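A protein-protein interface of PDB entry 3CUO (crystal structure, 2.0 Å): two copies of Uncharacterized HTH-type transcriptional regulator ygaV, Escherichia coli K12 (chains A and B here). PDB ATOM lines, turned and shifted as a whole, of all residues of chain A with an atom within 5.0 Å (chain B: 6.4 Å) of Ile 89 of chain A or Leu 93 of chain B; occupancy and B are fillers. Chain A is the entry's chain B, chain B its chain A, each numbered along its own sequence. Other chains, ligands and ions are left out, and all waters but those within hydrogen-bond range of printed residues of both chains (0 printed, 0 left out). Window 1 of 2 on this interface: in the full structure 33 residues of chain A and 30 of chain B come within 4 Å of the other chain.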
ATOM      1  N   LEU A   7      19.989  -3.275   4.268  1.00  0.00           N
ATOM      2  CA  LEU A   7      21.319  -3.841   4.402  1.00  0.00           C
ATOM      3  C   LEU A   7      22.283  -3.593   3.241  1.00  0.00           C
ATOM      4  O   LEU A   7      23.466  -3.848   3.376  1.00  0.00           O
ATOM      5  CB  LEU A   7      21.180  -5.375   4.632  1.00  0.00           C
ATOM      6  CG  LEU A   7      22.023  -6.060   5.716  1.00  0.00           C
ATOM      7  CD1 LEU A   7      21.857  -5.321   7.017  1.00  0.00           C
ATOM      8  CD2 LEU A   7      21.660  -7.555   5.884  1.00  0.00           C
ATOM      9  N   ALA A  14      29.514  -6.825   5.787  1.00  0.00           N
ATOM     10  CA  ALA A  14      28.860  -8.033   6.356  1.00  0.00           C
ATOM     11  C   ALA A  14      29.476  -9.285   5.757  1.00  0.00           C
ATOM     12  O   ALA A  14      29.863 -10.224   6.488  1.00  0.00           O
ATOM     13  CB  ALA A  14      27.333  -7.975   6.052  1.00  0.00           C
ATOM     14  N   LEU A  17      32.999  -9.938   7.134  1.00  0.00           N
ATOM     15  CA  LEU A  17      32.859 -10.487   8.446  1.00  0.00           C
ATOM     16  C   LEU A  17      32.507 -11.987   8.380  1.00  0.00           C
ATOM     17  O   LEU A  17      33.209 -12.858   8.987  1.00  0.00           O
ATOM     18  CB  LEU A  17      31.710  -9.706   9.187  1.00  0.00           C
ATOM     19  CG  LEU A  17      31.387 -10.283  10.604  1.00  0.00           C
ATOM     20  CD1 LEU A  17      32.594  -9.979  11.478  1.00  0.00           C
ATOM     21  CD2 LEU A  17      30.079  -9.791  11.278  1.00  0.00           C
ATOM     22  N   LEU A  18      31.450 -12.330   7.612  1.00  0.00           N
ATOM     23  CA  LEU A  18      31.043 -13.719   7.539  1.00  0.00           C
ATOM     24  C   LEU A  18      32.131 -14.566   6.959  1.00  0.00           C
ATOM     25  O   LEU A  18      32.376 -15.664   7.467  1.00  0.00           O
ATOM     26  CB  LEU A  18      29.735 -13.905   6.791  1.00  0.00           C
ATOM     27  CG  LEU A  18      28.510 -13.240   7.363  1.00  0.00           C
ATOM     28  CD1 LEU A  18      27.289 -13.741   6.565  1.00  0.00           C
ATOM     29  CD2 LEU A  18      28.399 -13.611   8.869  1.00  0.00           C
ATOM     30  N   MET A  21      34.842 -15.330   9.476  1.00  0.00           N
ATOM     31  CA  MET A  21      34.330 -16.304  10.471  1.00  0.00           C
ATOM     32  C   MET A  21      34.075 -17.714   9.910  1.00  0.00           C
ATOM     33  O   MET A  21      33.756 -18.614  10.650  1.00  0.00           O
ATOM     34  CB  MET A  21      33.006 -15.777  11.065  1.00  0.00           C
ATOM     35  CG  MET A  21      33.196 -14.441  11.864  1.00  0.00           C
ATOM     36  SD  MET A  21      31.661 -13.815  12.659  1.00  0.00           S
ATOM     37  CE  MET A  21      31.451 -15.231  13.842  1.00  0.00           C
ATOM     38  N   ALA A  85      30.325  -7.359  16.377  1.00  0.00           N
ATOM     39  CA  ALA A  85      29.580  -8.133  15.419  1.00  0.00           C
ATOM     40  C   ALA A  85      29.883  -9.654  15.536  1.00  0.00           C
ATOM     41  O   ALA A  85      29.001 -10.502  15.300  1.00  0.00           O
ATOM     42  CB  ALA A  85      29.810  -7.621  13.937  1.00  0.00           C
ATOM     43  N   VAL A  86      31.124  -9.997  15.878  1.00  0.00           N
ATOM     44  CA  VAL A  86      31.473 -11.411  16.054  1.00  0.00           C
ATOM     45  C   VAL A  86      30.650 -12.027  17.153  1.00  0.00           C
ATOM     46  O   VAL A  86      30.051 -13.125  17.009  1.00  0.00           O
ATOM     47  CB  VAL A  86      32.992 -11.577  16.333  1.00  0.00           C
ATOM     48  CG1 VAL A  86      33.261 -13.048  16.753  1.00  0.00           C
ATOM     49  CG2 VAL A  86      33.760 -11.133  15.087  1.00  0.00           C
ATOM     50  N   ASN A  87      30.639 -11.340  18.298  1.00  0.00           N
ATOM     51  CA  ASN A  87      29.827 -11.803  19.422  1.00  0.00           C
ATOM     52  C   ASN A  87      28.328 -11.892  19.060  1.00  0.00           C
ATOM     53  O   ASN A  87      27.590 -12.774  19.527  1.00  0.00           O
ATOM     54  CB  ASN A  87      29.990 -10.899  20.640  1.00  0.00           C
ATOM     55  CG  ASN A  87      31.385 -10.929  21.226  1.00  0.00           C
ATOM     56  OD1 ASN A  87      31.966  -9.903  21.506  1.00  0.00           O
ATOM     57  ND2 ASN A  87      31.931 -12.097  21.338  1.00  0.00           N
ATOM     58  N   ALA A  88      27.829 -10.969  18.276  1.00  0.00           N
ATOM     59  CA  ALA A  88      26.437 -11.086  17.871  1.00  0.00           C
ATOM     60  C   ALA A  88      26.200 -12.324  16.977  1.00  0.00           C
ATOM     61  O   ALA A  88      25.204 -13.074  17.123  1.00  0.00           O
ATOM     62  CB  ALA A  88      25.938  -9.811  17.220  1.00  0.00           C
ATOM     63  N   ILE A  89      27.112 -12.559  16.032  1.00  0.00           N
ATOM     64  CA  ILE A  89      26.932 -13.686  15.136  1.00  0.00           C
ATOM     65  C   ILE A  89      27.087 -15.012  15.921  1.00  0.00           C
ATOM     66  O   ILE A  89      26.311 -15.943  15.713  1.00  0.00           O
ATOM     67  CB  ILE A  89      27.910 -13.599  13.954  1.00  0.00           C
ATOM     68  CG1 ILE A  89      27.537 -12.414  13.015  1.00  0.00           C
ATOM     69  CG2 ILE A  89      28.075 -14.970  13.250  1.00  0.00           C
ATOM     70  CD1 ILE A  89      26.246 -12.643  12.117  1.00  0.00           C
ATOM     71  N   ILE A  90      28.071 -15.091  16.853  1.00  0.00           N
ATOM     72  CA  ILE A  90      28.216 -16.294  17.734  1.00  0.00           C
ATOM     73  C   ILE A  90      26.972 -16.633  18.547  1.00  0.00           C
ATOM     74  O   ILE A  90      26.560 -17.793  18.589  1.00  0.00           O
ATOM     75  CB  ILE A  90      29.390 -16.137  18.709  1.00  0.00           C
ATOM     76  CG1 ILE A  90      30.705 -16.321  17.944  1.00  0.00           C
ATOM     77  CG2 ILE A  90      29.301 -17.218  19.831  1.00  0.00           C
ATOM     78  CD1 ILE A  90      31.826 -15.834  18.689  1.00  0.00           C
ATOM     79  N   ALA A  91      26.336 -15.646  19.176  1.00  0.00           N
ATOM     80  CA  ALA A  91      25.022 -15.850  19.874  1.00  0.00           C
ATOM     81  C   ALA A  91      23.887 -16.348  18.983  1.00  0.00           C
ATOM     82  O   ALA A  91      23.096 -17.244  19.352  1.00  0.00           O
ATOM     83  CB  ALA A  91      24.599 -14.565  20.564  1.00  0.00           C
ATOM     84  N   THR A  92      23.784 -15.814  17.759  1.00  0.00           N
ATOM     85  CA  THR A  92      22.793 -16.340  16.837  1.00  0.00           C
ATOM     86  C   THR A  92      23.036 -17.801  16.473  1.00  0.00           C
ATOM     87  O   THR A  92      22.106 -18.565  16.348  1.00  0.00           O
ATOM     88  CB  THR A  92      22.690 -15.471  15.536  1.00  0.00           C
ATOM     89  OG1 THR A  92      22.351 -14.121  15.894  1.00  0.00           O
ATOM     90  CG2 THR A  92      21.642 -16.049  14.572  1.00  0.00           C
ATOM     91  N   LEU A  93      24.277 -18.148  16.197  1.00  0.00           N
ATOM     92  CA  LEU A  93      24.627 -19.490  15.818  1.00  0.00           C
ATOM     93  C   LEU A  93      24.273 -20.464  16.974  1.00  0.00           C
ATOM     94  O   LEU A  93      23.740 -21.547  16.781  1.00  0.00           O
ATOM     95  CB  LEU A  93      26.124 -19.544  15.437  1.00  0.00           C
ATOM     96  CG  LEU A  93      26.597 -18.880  14.141  1.00  0.00           C
ATOM     97  CD1 LEU A  93      28.145 -19.040  13.977  1.00  0.00           C
ATOM     98  CD2 LEU A  93      25.811 -19.423  12.988  1.00  0.00           C
ATOM     99  N   LEU B  18      28.043 -20.001   7.105  1.00  0.00           N
ATOM    100  CA  LEU B  18      28.585 -18.679   6.983  1.00  0.00           C
ATOM    101  C   LEU B  18      29.320 -18.539   5.660  1.00  0.00           C
ATOM    102  O   LEU B  18      29.230 -17.537   4.956  1.00  0.00           O
ATOM    103  CB  LEU B  18      29.506 -18.373   8.213  1.00  0.00           C
ATOM    104  CG  LEU B  18      28.912 -18.279   9.616  1.00  0.00           C
ATOM    105  CD1 LEU B  18      30.000 -17.693  10.516  1.00  0.00           C
ATOM    106  CD2 LEU B  18      27.610 -17.452   9.675  1.00  0.00           C
ATOM    107  N   MET B  21      26.975 -17.843   2.753  1.00  0.00           N
ATOM    108  CA  MET B  21      26.369 -16.548   2.785  1.00  0.00           C
ATOM    109  C   MET B  21      27.429 -15.447   2.579  1.00  0.00           C
ATOM    110  O   MET B  21      27.064 -14.305   2.447  1.00  0.00           O
ATOM    111  CB  MET B  21      25.735 -16.329   4.196  1.00  0.00           C
ATOM    112  CG  MET B  21      24.612 -17.348   4.591  1.00  0.00           C
ATOM    113  SD  MET B  21      23.703 -16.983   6.170  1.00  0.00           S
ATOM    114  CE  MET B  21      23.020 -15.394   5.915  1.00  0.00           C
ATOM    115  N   LEU B  27      24.141 -11.994  -0.120  1.00  0.00           N
ATOM    116  CA  LEU B  27      23.380 -11.369   0.953  1.00  0.00           C
ATOM    117  C   LEU B  27      22.231 -10.554   0.446  1.00  0.00           C
ATOM    118  O   LEU B  27      21.164 -10.586   1.041  1.00  0.00           O
ATOM    119  CB  LEU B  27      24.246 -10.448   1.874  1.00  0.00           C
ATOM    120  CG  LEU B  27      25.211 -11.164   2.789  1.00  0.00           C
ATOM    121  CD1 LEU B  27      25.985 -10.085   3.568  1.00  0.00           C
ATOM    122  CD2 LEU B  27      24.562 -12.226   3.769  1.00  0.00           C
ATOM    123  N   ALA B  88      17.706 -15.828  10.574  1.00  0.00           N
ATOM    124  CA  ALA B  88      18.370 -15.456  11.862  1.00  0.00           C
ATOM    125  C   ALA B  88      19.615 -14.637  11.659  1.00  0.00           C
ATOM    126  O   ALA B  88      19.866 -13.663  12.376  1.00  0.00           O
ATOM    127  CB  ALA B  88      18.703 -16.707  12.659  1.00  0.00           C
ATOM    128  N   ILE B  89      20.455 -15.050  10.702  1.00  0.00           N
ATOM    129  CA  ILE B  89      21.710 -14.351  10.469  1.00  0.00           C
ATOM    130  C   ILE B  89      21.445 -13.009   9.833  1.00  0.00           C
ATOM    131  O   ILE B  89      22.024 -11.984  10.227  1.00  0.00           O
ATOM    132  CB  ILE B  89      22.643 -15.223   9.654  1.00  0.00           C
ATOM    133  CG1 ILE B  89      23.054 -16.382  10.541  1.00  0.00           C
ATOM    134  CG2 ILE B  89      23.867 -14.393   9.066  1.00  0.00           C
ATOM    135  CD1 ILE B  89      23.511 -17.558   9.836  1.00  0.00           C
ATOM    136  N   ILE B  90      20.587 -12.984   8.815  1.00  0.00           N
ATOM    137  CA  ILE B  90      20.144 -11.728   8.244  1.00  0.00           C
ATOM    138  C   ILE B  90      19.645 -10.707   9.265  1.00  0.00           C
ATOM    139  O   ILE B  90      20.023  -9.546   9.238  1.00  0.00           O
ATOM    140  CB  ILE B  90      19.057 -11.976   7.095  1.00  0.00           C
ATOM    141  CG1 ILE B  90      19.772 -12.536   5.873  1.00  0.00           C
ATOM    142  CG2 ILE B  90      18.364 -10.700   6.780  1.00  0.00           C
ATOM    143  CD1 ILE B  90      18.883 -12.487   4.563  1.00  0.00           C
ATOM    144  N   ALA B  91      18.803 -11.151  10.171  1.00  0.00           N
ATOM    145  CA  ALA B  91      18.242 -10.289  11.197  1.00  0.00           C
ATOM    146  C   ALA B  91      19.344  -9.782  12.146  1.00  0.00           C
ATOM    147  O   ALA B  91      19.344  -8.587  12.536  1.00  0.00           O
ATOM    148  CB  ALA B  91      17.177 -11.074  11.973  1.00  0.00           C
ATOM    149  N   THR B  92      20.314 -10.636  12.494  1.00  0.00           N
ATOM    150  CA  THR B  92      21.460 -10.143  13.296  1.00  0.00           C
ATOM    151  C   THR B  92      22.303  -9.143  12.499  1.00  0.00           C
ATOM    152  O   THR B  92      22.764  -8.135  13.050  1.00  0.00           O
ATOM    153  CB  THR B  92      22.303 -11.329  13.774  1.00  0.00           C
ATOM    154  OG1 THR B  92      21.477 -12.153  14.605  1.00  0.00           O
ATOM    155  CG2 THR B  92      23.526 -10.907  14.557  1.00  0.00           C
ATOM    156  N   LEU B  93      22.529  -9.410  11.204  1.00  0.00           N
ATOM    157  CA  LEU B  93      23.327  -8.487  10.414  1.00  0.00           C
ATOM    158  C   LEU B  93      22.640  -7.112  10.358  1.00  0.00           C
ATOM    159  O   LEU B  93      23.269  -6.069  10.487  1.00  0.00           O
ATOM    160  CB  LEU B  93      23.582  -9.037   9.024  1.00  0.00           C
ATOM    161  CG  LEU B  93      24.520 -10.234   8.899  1.00  0.00           C
ATOM    162  CD1 LEU B  93      24.512 -10.670   7.480  1.00  0.00           C
ATOM    163  CD2 LEU B  93      25.905  -9.923   9.293  1.00  0.00           C
ATOM    164  N   LYS B  94      21.336  -7.117  10.134  1.00  0.00           N
ATOM    165  CA  LYS B  94      20.528  -5.900  10.287  1.00  0.00           C
ATOM    166  C   LYS B  94      20.780  -5.153  11.588  1.00  0.00           C
ATOM    167  O   LYS B  94      21.098  -3.971  11.542  1.00  0.00           O
ATOM    168  CB  LYS B  94      19.014  -6.151  10.064  1.00  0.00           C
ATOM    169  CG  LYS B  94      18.679  -6.512   8.619  1.00  0.00           C
ATOM    170  CD  LYS B  94      17.121  -6.846   8.373  1.00  0.00           C
ATOM    171  CE  LYS B  94      16.823  -8.331   8.067  1.00  0.00           C
ATOM    172  NZ  LYS B  94      15.348  -8.833   8.189  1.00  0.00           N
ATOM    173  N   ASN B  95      20.645  -5.818  12.733  1.00  0.00           N
ATOM    174  CA  ASN B  95      20.894  -5.209  14.044  1.00  0.00           C
ATOM    175  C   ASN B  95      22.292  -4.665  14.178  1.00  0.00           C
ATOM    176  O   ASN B  95      22.485  -3.603  14.772  1.00  0.00           O
ATOM    177  CB  ASN B  95      20.637  -6.210  15.186  1.00  0.00           C
ATOM    178  CG  ASN B  95      19.178  -6.423  15.455  1.00  0.00           C
ATOM    179  OD1 ASN B  95      18.379  -5.510  15.292  1.00  0.00           O
ATOM    180  ND2 ASN B  95      18.809  -7.640  15.875  1.00  0.00           N
ATOM    181  N   VAL B  96      23.266  -5.336  13.575  1.00  0.00           N
ATOM    182  CA  VAL B  96      24.665  -4.923  13.677  1.00  0.00           C
ATOM    183  C   VAL B  96      24.957  -3.674  12.804  1.00  0.00           C
ATOM    184  O   VAL B  96      25.589  -2.730  13.238  1.00  0.00           O
ATOM    185  CB  VAL B  96      25.620  -6.131  13.314  1.00  0.00           C
ATOM    186  CG1 VAL B  96      27.023  -5.696  13.030  1.00  0.00           C
ATOM    187  CG2 VAL B  96      25.580  -7.203  14.436  1.00  0.00           C
ATOM    188  N   TYR B  97      24.509  -3.719  11.565  1.00  0.00           N
ATOM    189  CA  TYR B  97      24.887  -2.751  10.541  1.00  0.00           C
ATOM    190  C   TYR B  97      23.877  -1.657  10.295  1.00  0.00           C
ATOM    191  O   TYR B  97      24.185  -0.719   9.591  1.00  0.00           O
ATOM    192  CB  TYR B  97      25.150  -3.469   9.231  1.00  0.00           C
ATOM    193  CG  TYR B  97      26.389  -4.296   9.286  1.00  0.00           C
ATOM    194  CD1 TYR B  97      27.634  -3.685   9.267  1.00  0.00           C
ATOM    195  CD2 TYR B  97      26.334  -5.688   9.374  1.00  0.00           C
ATOM    196  CE1 TYR B  97      28.781  -4.420   9.320  1.00  0.00           C
ATOM    197  CE2 TYR B  97      27.490  -6.443   9.462  1.00  0.00           C
ATOM    198  CZ  TYR B  97      28.730  -5.784   9.406  1.00  0.00           C
ATOM    199  OH  TYR B  97      29.912  -6.497   9.485  1.00  0.00           O
ATOM    200  N   CYS B  98      22.678  -1.781  10.851  1.00  0.00           N
ATOM    201  CA  CYS B  98      21.596  -0.805  10.622  1.00  0.00           C
ATOM    202  C   CYS B  98      21.221  -0.138  11.950  1.00  0.00           C
ATOM    203  O   CYS B  98      20.709  -0.804  12.865  1.00  0.00           O
ATOM    204  CB  CYS B  98      20.356  -1.476   9.987  1.00  0.00           C
ATOM    205  SG  CYS B  98      20.692  -2.384   8.371  1.00  0.00           S
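The side-chain hydroxyl (OG1) of Thr 92 of chain A sits at hydrogen-bond distance from the side-chain hydroxyl (OG1) of Thr 92 of chain B (2.5 Å).
O of Ala 88 of chain B sits at hydrogen-bond distance from OG1 of Thr 92 of chain B, at 3.1 Å. The side-chain sulfur (SG) of Cys 98 of chain B lies close to the backbone carbonyl oxygen (O) of Lys 94 of chain B, at 3.6 Å. O of Ala 88 of chain A is in hydrogen-bond range of OG1 of Thr 92 of chain A, 3.3 Å away.
Among the printed residues, merely in contact across the chains: Leu 7 of chain A with Cys 98 of chain B, Ala 85 of chain A with Val 96 of chain B, Ala 14 of chain A with Leu 27 of chain B, Thr 92 of chain A with Ala 88 of chain B, Leu 7 of chain A with Lys 94 of chain B, Met 21 of chain A with Leu 18 of chain B, Ala 14 of chain A with Tyr 97 of chain B, Leu 17 of chain A with Tyr 97 of chain B, Ala 88 of chain A with Thr 92 of chain B, Leu 7 of chain A with Leu 93 of chain B, Ala 88 of chain A with Val 96 of chain B, Leu 18 of chain A with Met 21 of chain B and Ile 89 of chain A with Leu 93 of chain B.
Printed residues of chain B within 4 Å of Met 21 of chain A: Leu 18 (3.6 Å). Of the printed residues of chain A, Ala 88 of chain B touches Thr 92 (3.6 Å). Of chain A, only Leu 7 (3.8 Å) and Ile 89 (3.9 Å) come within 4 Å of Leu 93 of chain B. Of the printed residues of chain A, Lys 94 of chain B touches Leu 7. Of the printed residues of chain A, Tyr 97 of chain B touches Ala 14 (3.6 Å) and Leu 17 (3.7 Å). The nearest residue of chain B that does not touch Ile 89 of chain A is Thr 92 of chain B (4.05 Å). The nearest residue of chain A that does not touch Leu 93 of chain B is Ala 14 of chain A (4.04 Å).
Hydrophobic or aromatic side chains of chain A within 4 Å of the printed part of chain B: Leu 7, Ala 14, Leu 17, Leu 18, Met 21, Ala 85, Ala 88 and Ile 89. Of the 14 printed residues of chain B, 10 touch a printed residue of chain A. Hydrophobic or aromatic side chains of chain B that line the printed part of chain A: Leu 18, Met 21, Leu 27, Ala 88, Leu 93, Val 96 and Tyr 97.
Leu 18 of chain A touches Met 21 of chain B, and with the chains exchanged Met 21 of chain A touches Leu 18 of chain B. Ala 88 of chain A touches Thr 92 of chain B, and with the chains exchanged Thr 92 of chain A touches Ala 88 of chain B. Ile 89 of chain A touches Leu 93 of chain B, but with the chains exchanged Leu 93 of chain A does not touch Ile 89 of chain B (4.3 Å). Thr 92 of chain A touches its own counterpart, Thr 92 of chain B. Of the 14 pairs that touch across the chains among the printed residues, 5 have their exchanged pair printed and touching as well.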
